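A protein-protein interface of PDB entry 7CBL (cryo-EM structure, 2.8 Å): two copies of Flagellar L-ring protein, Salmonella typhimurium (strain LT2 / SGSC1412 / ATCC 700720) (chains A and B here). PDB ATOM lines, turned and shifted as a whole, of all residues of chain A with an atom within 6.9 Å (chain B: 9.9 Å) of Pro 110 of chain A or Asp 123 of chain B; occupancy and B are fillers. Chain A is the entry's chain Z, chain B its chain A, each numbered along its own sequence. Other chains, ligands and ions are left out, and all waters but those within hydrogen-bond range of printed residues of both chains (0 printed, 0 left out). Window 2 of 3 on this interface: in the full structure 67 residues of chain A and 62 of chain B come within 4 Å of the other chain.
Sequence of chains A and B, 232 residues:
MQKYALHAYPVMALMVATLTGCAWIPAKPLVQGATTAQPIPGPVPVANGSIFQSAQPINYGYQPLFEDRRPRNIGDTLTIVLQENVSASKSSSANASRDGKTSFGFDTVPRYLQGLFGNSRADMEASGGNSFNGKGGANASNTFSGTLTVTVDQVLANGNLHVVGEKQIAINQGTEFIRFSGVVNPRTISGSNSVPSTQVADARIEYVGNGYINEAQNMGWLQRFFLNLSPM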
ATOM      1  N   PHE A 106     -30.331  -4.879  -2.503  1.00  0.00           N
ATOM      2  CA  PHE A 106     -29.466  -3.769  -2.886  1.00  0.00           C
ATOM      3  C   PHE A 106     -28.515  -4.273  -3.961  1.00  0.00           C
ATOM      4  O   PHE A 106     -27.526  -4.945  -3.666  1.00  0.00           O
ATOM      5  CB  PHE A 106     -28.712  -3.245  -1.674  1.00  0.00           C
ATOM      6  CG  PHE A 106     -28.644  -1.761  -1.602  1.00  0.00           C
ATOM      7  CD1 PHE A 106     -28.361  -1.017  -2.726  1.00  0.00           C
ATOM      8  CD2 PHE A 106     -28.863  -1.106  -0.411  1.00  0.00           C
ATOM      9  CE1 PHE A 106     -28.296   0.351  -2.660  1.00  0.00           C
ATOM     10  CE2 PHE A 106     -28.800   0.261  -0.341  1.00  0.00           C
ATOM     11  CZ  PHE A 106     -28.516   0.991  -1.466  1.00  0.00           C
ATOM     12  N   THR A 108     -26.594  -2.529  -6.557  1.00  0.00           N
ATOM     13  CA  THR A 108     -25.341  -1.792  -6.640  1.00  0.00           C
ATOM     14  C   THR A 108     -25.285  -0.822  -5.472  1.00  0.00           C
ATOM     15  O   THR A 108     -26.055   0.141  -5.424  1.00  0.00           O
ATOM     16  CB  THR A 108     -25.228  -1.052  -7.967  1.00  0.00           C
ATOM     17  OG1 THR A 108     -25.327  -1.989  -9.046  1.00  0.00           O
ATOM     18  CG2 THR A 108     -23.907  -0.322  -8.057  1.00  0.00           C
ATOM     19  N   VAL A 109     -24.382  -1.072  -4.534  1.00  0.00           N
ATOM     20  CA  VAL A 109     -24.262  -0.225  -3.354  1.00  0.00           C
ATOM     21  C   VAL A 109     -23.237   0.864  -3.630  1.00  0.00           C
ATOM     22  O   VAL A 109     -22.130   0.565  -4.097  1.00  0.00           O
ATOM     23  CB  VAL A 109     -23.869  -1.044  -2.118  1.00  0.00           C
ATOM     24  CG1 VAL A 109     -24.113  -0.242  -0.859  1.00  0.00           C
ATOM     25  CG2 VAL A 109     -24.637  -2.344  -2.085  1.00  0.00           C
ATOM     26  N   PRO A 110     -23.551   2.129  -3.368  1.00  0.00           N
ATOM     27  CA  PRO A 110     -22.528   3.170  -3.467  1.00  0.00           C
ATOM     28  C   PRO A 110     -21.439   2.949  -2.431  1.00  0.00           C
ATOM     29  O   PRO A 110     -21.597   2.189  -1.476  1.00  0.00           O
ATOM     30  CB  PRO A 110     -23.306   4.461  -3.198  1.00  0.00           C
ATOM     31  CG  PRO A 110     -24.499   4.025  -2.438  1.00  0.00           C
ATOM     32  CD  PRO A 110     -24.858   2.681  -2.983  1.00  0.00           C
ATOM     33  N   ARG A 111     -20.315   3.634  -2.632  1.00  0.00           N
ATOM     34  CA  ARG A 111     -19.156   3.412  -1.775  1.00  0.00           C
ATOM     35  C   ARG A 111     -19.443   3.825  -0.338  1.00  0.00           C
ATOM     36  O   ARG A 111     -19.180   3.067   0.601  1.00  0.00           O
ATOM     37  CB  ARG A 111     -17.950   4.169  -2.325  1.00  0.00           C
ATOM     38  CG  ARG A 111     -16.657   3.868  -1.600  1.00  0.00           C
ATOM     39  CD  ARG A 111     -15.465   4.366  -2.390  1.00  0.00           C
ATOM     40  NE  ARG A 111     -15.385   3.734  -3.702  1.00  0.00           N
ATOM     41  CZ  ARG A 111     -14.534   4.096  -4.654  1.00  0.00           C
ATOM     42  NH1 ARG A 111     -13.685   5.092  -4.442  1.00  0.00           N
ATOM     43  NH2 ARG A 111     -14.529   3.464  -5.820  1.00  0.00           N
ATOM     44  N   TYR A 112     -19.998   5.022  -0.147  1.00  0.00           N
ATOM     45  CA  TYR A 112     -20.217   5.540   1.197  1.00  0.00           C
ATOM     46  C   TYR A 112     -21.257   4.753   1.980  1.00  0.00           C
ATOM     47  O   TYR A 112     -21.437   5.020   3.172  1.00  0.00           O
ATOM     48  CB  TYR A 112     -20.624   7.010   1.138  1.00  0.00           C
ATOM     49  CG  TYR A 112     -21.899   7.267   0.376  1.00  0.00           C
ATOM     50  CD1 TYR A 112     -21.890   7.403  -1.002  1.00  0.00           C
ATOM     51  CD2 TYR A 112     -23.112   7.383   1.036  1.00  0.00           C
ATOM     52  CE1 TYR A 112     -23.049   7.639  -1.701  1.00  0.00           C
ATOM     53  CE2 TYR A 112     -24.278   7.620   0.343  1.00  0.00           C
ATOM     54  CZ  TYR A 112     -24.239   7.746  -1.025  1.00  0.00           C
ATOM     55  OH  TYR A 112     -25.395   7.982  -1.726  1.00  0.00           O
ATOM     56  N   LEU A 113     -21.943   3.804   1.352  1.00  0.00           N
ATOM     57  CA  LEU A 113     -22.878   2.932   2.045  1.00  0.00           C
ATOM     58  C   LEU A 113     -22.371   1.505   2.159  1.00  0.00           C
ATOM     59  O   LEU A 113     -23.069   0.661   2.727  1.00  0.00           O
ATOM     60  CB  LEU A 113     -24.234   2.934   1.334  1.00  0.00           C
ATOM     61  CG  LEU A 113     -25.101   4.171   1.544  1.00  0.00           C
ATOM     62  CD1 LEU A 113     -26.427   4.009   0.837  1.00  0.00           C
ATOM     63  CD2 LEU A 113     -25.309   4.416   3.021  1.00  0.00           C
ATOM     64  N   GLN A 114     -21.173   1.216   1.644  1.00  0.00           N
ATOM     65  CA  GLN A 114     -20.680  -0.156   1.634  1.00  0.00           C
ATOM     66  C   GLN A 114     -20.564  -0.724   3.039  1.00  0.00           C
ATOM     67  O   GLN A 114     -20.641  -1.943   3.224  1.00  0.00           O
ATOM     68  CB  GLN A 114     -19.331  -0.220   0.926  1.00  0.00           C
ATOM     69  CG  GLN A 114     -18.988  -1.592   0.394  1.00  0.00           C
ATOM     70  CD  GLN A 114     -19.638  -1.870  -0.940  1.00  0.00           C
ATOM     71  OE1 GLN A 114     -20.043  -2.996  -1.224  1.00  0.00           O
ATOM     72  NE2 GLN A 114     -19.739  -0.844  -1.772  1.00  0.00           N
ATOM     73  N   GLY A 115     -20.387   0.132   4.038  1.00  0.00           N
ATOM     74  CA  GLY A 115     -20.307  -0.329   5.406  1.00  0.00           C
ATOM     75  C   GLY A 115     -21.618  -0.756   6.021  1.00  0.00           C
ATOM     76  O   GLY A 115     -21.630  -1.160   7.186  1.00  0.00           O
ATOM     77  N   THR B 102     -35.196   2.275  -6.936  1.00  0.00           N
ATOM     78  CA  THR B 102     -34.427   3.492  -7.125  1.00  0.00           C
ATOM     79  C   THR B 102     -33.111   3.173  -7.818  1.00  0.00           C
ATOM     80  O   THR B 102     -32.599   2.055  -7.742  1.00  0.00           O
ATOM     81  CB  THR B 102     -34.161   4.198  -5.795  1.00  0.00           C
ATOM     82  OG1 THR B 102     -33.363   5.362  -6.028  1.00  0.00           O
ATOM     83  CG2 THR B 102     -33.432   3.284  -4.848  1.00  0.00           C
ATOM     84  N   SER B 103     -32.560   4.179  -8.492  1.00  0.00           N
ATOM     85  CA  SER B 103     -31.359   3.984  -9.288  1.00  0.00           C
ATOM     86  C   SER B 103     -30.716   5.330  -9.578  1.00  0.00           C
ATOM     87  O   SER B 103     -31.373   6.371  -9.559  1.00  0.00           O
ATOM     88  CB  SER B 103     -31.669   3.263 -10.597  1.00  0.00           C
ATOM     89  OG  SER B 103     -30.851   3.758 -11.637  1.00  0.00           O
ATOM     90  N   PHE B 104     -29.414   5.285  -9.847  1.00  0.00           N
ATOM     91  CA  PHE B 104     -28.655   6.464 -10.242  1.00  0.00           C
ATOM     92  C   PHE B 104     -27.303   6.050 -10.796  1.00  0.00           C
ATOM     93  O   PHE B 104     -26.599   5.248 -10.180  1.00  0.00           O
ATOM     94  CB  PHE B 104     -28.454   7.416  -9.069  1.00  0.00           C
ATOM     95  CG  PHE B 104     -27.480   8.513  -9.353  1.00  0.00           C
ATOM     96  CD1 PHE B 104     -27.775   9.491 -10.280  1.00  0.00           C
ATOM     97  CD2 PHE B 104     -26.268   8.569  -8.700  1.00  0.00           C
ATOM     98  CE1 PHE B 104     -26.885  10.501 -10.548  1.00  0.00           C
ATOM     99  CE2 PHE B 104     -25.374   9.580  -8.966  1.00  0.00           C
ATOM    100  CZ  PHE B 104     -25.684  10.546  -9.890  1.00  0.00           C
ATOM    101  N   GLY B 105     -26.929   6.585 -11.951  1.00  0.00           N
ATOM    102  CA  GLY B 105     -25.664   6.213 -12.547  1.00  0.00           C
ATOM    103  C   GLY B 105     -24.996   7.318 -13.332  1.00  0.00           C
ATOM    104  O   GLY B 105     -25.569   7.852 -14.283  1.00  0.00           O
ATOM    105  N   PHE B 106     -23.769   7.655 -12.950  1.00  0.00           N
ATOM    106  CA  PHE B 106     -22.971   8.656 -13.650  1.00  0.00           C
ATOM    107  C   PHE B 106     -22.138   7.933 -14.697  1.00  0.00           C
ATOM    108  O   PHE B 106     -21.113   7.331 -14.382  1.00  0.00           O
ATOM    109  CB  PHE B 106     -22.095   9.415 -12.665  1.00  0.00           C
ATOM    110  CG  PHE B 106     -22.044  10.882 -12.913  1.00  0.00           C
ATOM    111  CD1 PHE B 106     -21.902  11.373 -14.190  1.00  0.00           C
ATOM    112  CD2 PHE B 106     -22.139  11.772 -11.865  1.00  0.00           C
ATOM    113  CE1 PHE B 106     -21.852  12.726 -14.418  1.00  0.00           C
ATOM    114  CE2 PHE B 106     -22.091  13.123 -12.087  1.00  0.00           C
ATOM    115  CZ  PHE B 106     -21.948  13.601 -13.365  1.00  0.00           C
ATOM    116  N   ASP B 107     -22.582   7.988 -15.951  1.00  0.00           N
ATOM    117  CA  ASP B 107     -21.918   7.232 -17.006  1.00  0.00           C
ATOM    118  C   ASP B 107     -20.561   7.838 -17.344  1.00  0.00           C
ATOM    119  O   ASP B 107     -19.523   7.185 -17.204  1.00  0.00           O
ATOM    120  CB  ASP B 107     -22.819   7.176 -18.239  1.00  0.00           C
ATOM    121  CG  ASP B 107     -22.328   6.194 -19.286  1.00  0.00           C
ATOM    122  OD1 ASP B 107     -21.101   6.038 -19.450  1.00  0.00           O
ATOM    123  OD2 ASP B 107     -23.179   5.572 -19.952  1.00  0.00           O
ATOM    124  N   THR B 108     -20.551   9.085 -17.800  1.00  0.00           N
ATOM    125  CA  THR B 108     -19.327   9.781 -18.176  1.00  0.00           C
ATOM    126  C   THR B 108     -19.157  10.971 -17.248  1.00  0.00           C
ATOM    127  O   THR B 108     -19.932  11.929 -17.312  1.00  0.00           O
ATOM    128  CB  THR B 108     -19.376  10.227 -19.631  1.00  0.00           C
ATOM    129  OG1 THR B 108     -19.580   9.087 -20.473  1.00  0.00           O
ATOM    130  CG2 THR B 108     -18.086  10.912 -20.019  1.00  0.00           C
ATOM    131  N   VAL B 109     -18.150  10.915 -16.387  1.00  0.00           N
ATOM    132  CA  VAL B 109     -17.913  11.988 -15.429  1.00  0.00           C
ATOM    133  C   VAL B 109     -16.942  12.989 -16.039  1.00  0.00           C
ATOM    134  O   VAL B 109     -15.890  12.592 -16.556  1.00  0.00           O
ATOM    135  CB  VAL B 109     -17.369  11.442 -14.102  1.00  0.00           C
ATOM    136  CG1 VAL B 109     -17.485  12.489 -13.018  1.00  0.00           C
ATOM    137  CG2 VAL B 109     -18.107  10.183 -13.715  1.00  0.00           C
ATOM    138  N   LEU B 116     -15.399  13.331  -7.113  1.00  0.00           N
ATOM    139  CA  LEU B 116     -16.614  13.081  -6.345  1.00  0.00           C
ATOM    140  C   LEU B 116     -17.449  11.938  -6.895  1.00  0.00           C
ATOM    141  O   LEU B 116     -18.067  11.212  -6.117  1.00  0.00           O
ATOM    142  CB  LEU B 116     -17.463  14.353  -6.284  1.00  0.00           C
ATOM    143  CG  LEU B 116     -16.950  15.441  -5.343  1.00  0.00           C
ATOM    144  CD1 LEU B 116     -16.181  16.493  -6.119  1.00  0.00           C
ATOM    145  CD2 LEU B 116     -18.101  16.069  -4.587  1.00  0.00           C
ATOM    146  N   PHE B 117     -17.488  11.760  -8.211  1.00  0.00           N
ATOM    147  CA  PHE B 117     -18.319  10.734  -8.822  1.00  0.00           C
ATOM    148  C   PHE B 117     -17.516   9.776  -9.688  1.00  0.00           C
ATOM    149  O   PHE B 117     -18.100   9.038 -10.487  1.00  0.00           O
ATOM    150  CB  PHE B 117     -19.431  11.380  -9.648  1.00  0.00           C
ATOM    151  CG  PHE B 117     -20.292  12.330  -8.868  1.00  0.00           C
ATOM    152  CD1 PHE B 117     -19.963  13.669  -8.776  1.00  0.00           C
ATOM    153  CD2 PHE B 117     -21.434  11.886  -8.232  1.00  0.00           C
ATOM    154  CE1 PHE B 117     -20.752  14.541  -8.061  1.00  0.00           C
ATOM    155  CE2 PHE B 117     -22.225  12.755  -7.516  1.00  0.00           C
ATOM    156  CZ  PHE B 117     -21.884  14.082  -7.431  1.00  0.00           C
ATOM    157  N   GLY B 118     -16.196   9.775  -9.562  1.00  0.00           N
ATOM    158  CA  GLY B 118     -15.383   8.899 -10.372  1.00  0.00           C
ATOM    159  C   GLY B 118     -15.308   7.491  -9.820  1.00  0.00           C
ATOM    160  O   GLY B 118     -15.570   7.238  -8.647  1.00  0.00           O
ATOM    161  N   ASN B 119     -14.925   6.562 -10.698  1.00  0.00           N
ATOM    162  CA  ASN B 119     -14.798   5.145 -10.355  1.00  0.00           C
ATOM    163  C   ASN B 119     -16.113   4.565  -9.845  1.00  0.00           C
ATOM    164  O   ASN B 119     -16.116   3.652  -9.014  1.00  0.00           O
ATOM    165  CB  ASN B 119     -13.678   4.899  -9.335  1.00  0.00           C
ATOM    166  CG  ASN B 119     -12.430   5.714  -9.620  1.00  0.00           C
ATOM    167  OD1 ASN B 119     -11.462   5.204 -10.182  1.00  0.00           O
ATOM    168  ND2 ASN B 119     -12.432   6.973  -9.203  1.00  0.00           N
ATOM    169  N   SER B 120     -17.234   5.092 -10.338  1.00  0.00           N
ATOM    170  CA  SER B 120     -18.567   4.625  -9.966  1.00  0.00           C
ATOM    171  C   SER B 120     -18.784   4.666  -8.457  1.00  0.00           C
ATOM    172  O   SER B 120     -19.525   3.855  -7.903  1.00  0.00           O
ATOM    173  CB  SER B 120     -18.831   3.218 -10.506  1.00  0.00           C
ATOM    174  OG  SER B 120     -18.456   3.123 -11.869  1.00  0.00           O
ATOM    175  N   ARG B 121     -18.152   5.621  -7.782  1.00  0.00           N
ATOM    176  CA  ARG B 121     -18.238   5.710  -6.333  1.00  0.00           C
ATOM    177  C   ARG B 121     -19.561   6.283  -5.849  1.00  0.00           C
ATOM    178  O   ARG B 121     -19.768   6.378  -4.635  1.00  0.00           O
ATOM    179  CB  ARG B 121     -17.088   6.554  -5.792  1.00  0.00           C
ATOM    180  CG  ARG B 121     -17.307   8.041  -5.927  1.00  0.00           C
ATOM    181  CD  ARG B 121     -15.991   8.781  -5.837  1.00  0.00           C
ATOM    182  NE  ARG B 121     -15.208   8.355  -4.685  1.00  0.00           N
ATOM    183  CZ  ARG B 121     -13.888   8.467  -4.601  1.00  0.00           C
ATOM    184  NH1 ARG B 121     -13.201   8.989  -5.606  1.00  0.00           N
ATOM    185  NH2 ARG B 121     -13.257   8.054  -3.511  1.00  0.00           N
ATOM    186  N   ALA B 122     -20.452   6.671  -6.756  1.00  0.00           N
ATOM    187  CA  ALA B 122     -21.757   7.183  -6.374  1.00  0.00           C
ATOM    188  C   ALA B 122     -22.915   6.464  -7.039  1.00  0.00           C
ATOM    189  O   ALA B 122     -24.066   6.764  -6.709  1.00  0.00           O
ATOM    190  CB  ALA B 122     -21.861   8.681  -6.685  1.00  0.00           C
ATOM    191  N   ASP B 123     -22.657   5.537  -7.957  1.00  0.00           N
ATOM    192  CA  ASP B 123     -23.735   4.784  -8.578  1.00  0.00           C
ATOM    193  C   ASP B 123     -24.507   4.007  -7.524  1.00  0.00           C
ATOM    194  O   ASP B 123     -23.970   3.625  -6.484  1.00  0.00           O
ATOM    195  CB  ASP B 123     -23.183   3.836  -9.636  1.00  0.00           C
ATOM    196  CG  ASP B 123     -22.513   4.567 -10.774  1.00  0.00           C
ATOM    197  OD1 ASP B 123     -22.169   5.752 -10.591  1.00  0.00           O
ATOM    198  OD2 ASP B 123     -22.332   3.964 -11.850  1.00  0.00           O
ATOM    199  N   MET B 124     -25.785   3.778  -7.801  1.00  0.00           N
ATOM    200  CA  MET B 124     -26.672   3.188  -6.814  1.00  0.00           C
ATOM    201  C   MET B 124     -27.813   2.502  -7.538  1.00  0.00           C
ATOM    202  O   MET B 124     -28.233   2.941  -8.608  1.00  0.00           O
ATOM    203  CB  MET B 124     -27.202   4.255  -5.853  1.00  0.00           C
ATOM    204  CG  MET B 124     -28.066   3.727  -4.736  1.00  0.00           C
ATOM    205  SD  MET B 124     -29.816   3.789  -5.143  1.00  0.00           S
ATOM    206  CE  MET B 124     -29.974   5.497  -5.648  1.00  0.00           C
ATOM    207  N   GLU B 125     -28.309   1.421  -6.944  1.00  0.00           N
ATOM    208  CA  GLU B 125     -29.439   0.695  -7.515  1.00  0.00           C
ATOM    209  C   GLU B 125     -30.031  -0.196  -6.440  1.00  0.00           C
ATOM    210  O   GLU B 125     -29.321  -1.030  -5.875  1.00  0.00           O
ATOM    211  CB  GLU B 125     -29.003  -0.125  -8.713  1.00  0.00           C
ATOM    212  CG  GLU B 125     -30.046  -1.101  -9.179  1.00  0.00           C
ATOM    213  CD  GLU B 125     -29.853  -1.491 -10.623  1.00  0.00           C
ATOM    214  OE1 GLU B 125     -29.095  -0.794 -11.326  1.00  0.00           O
ATOM    215  OE2 GLU B 125     -30.457  -2.493 -11.057  1.00  0.00           O
ATOM    216  N   ALA B 126     -31.319  -0.030  -6.156  1.00  0.00           N
ATOM    217  CA  ALA B 126     -31.972  -0.792  -5.107  1.00  0.00           C
ATOM    218  C   ALA B 126     -33.412  -1.078  -5.494  1.00  0.00           C
ATOM    219  O   ALA B 126     -34.030  -0.326  -6.249  1.00  0.00           O
ATOM    220  CB  ALA B 126     -31.934  -0.058  -3.767  1.00  0.00           C
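Hydrophobic or aromatic side chains of chain A that line the printed part of chain B: Phe 106 and Pro 110.
Among the printed residues, 9 pairs touch across the chains.
Among the printed residues, no Asp or Glu carboxylate lies within 4 Å of a Lys or Arg side-chain nitrogen of the other chain.
N of Ala 126 of chain B sits at hydrogen-bond distance from O of Thr 102 of chain B, at 2.9 Å.
N of Phe 104 of chain B is in hydrogen-bond range of O of Met 124 of chain B (2.9 Å).
The side-chain carboxylate of Asp 123 of chain B sits at hydrogen-bond distance from the backbone NH of Phe 106 of chain B (3.4 Å).
Among the printed residues, merely in contact across the chains: Phe 106 of chain A with Met 124 of chain B (3.97 Å), Phe 106 of chain A with Glu 125 of chain B (3.3 Å), Phe 106 of chain A with Ala 126 of chain B (3.8 Å), Thr 108 of chain A with Met 124 of chain B (3.4 Å), Pro 110 of chain A with Met 124 of chain B (3.8 Å) and Arg 111 of chain A with Asn 119 of chain B (3.6 Å).
N of Arg 111 of chain A is in hydrogen-bond range of O of Arg 121 of chain B (3.4 Å).
The backbone NH (N) of Glu 125 of chain B lies within hydrogen-bond range of the backbone carbonyl oxygen (O) of Thr 108 of chain A, 3.0 Å away.
The backbone nitrogen (N) of Pro 110 of chain A sits close to the backbone carbonyl oxygen (O) of Asp 123 of chain B, 3.5 Å away.
Printed residues of chain B within 4 Å of Thr 108 of chain A: Met 124 (3.4 Å) and Glu 125 (3.0 Å).
No residue of chain B comes within 4 Å of Val 109 of chain A.
Of chain B, only Asp 123 (3.4 Å) and Met 124 (3.8 Å) come within 4 Å of Pro 110 of chain A.
No residue of chain B comes within 4 Å of Tyr 112 of chain A.
No residue of chain B comes within 4 Å of Leu 113 of chain A.
Of the printed residues of chain A, Asn 119 of chain B touches Arg 111 (3.6 Å).
Printed residues of chain A within 4 Å of Arg 121 of chain B: Arg 111.
Of chain A, only Pro 110 (3.4 Å) comes within 4 Å of Asp 123 of chain B.
Of the printed residues of chain A, Met 124 of chain B touches Phe 106 (3.97 Å), Thr 108 (3.4 Å) and Pro 110 (3.8 Å).
Of the printed residues of chain A, Ala 126 of chain B touches Phe 106.
Positions printed for both chains: 106, 108 and 109.
Of the 9 pairs that touch across the chains among the printed residues, none has its exchanged pair printed and touching as well.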
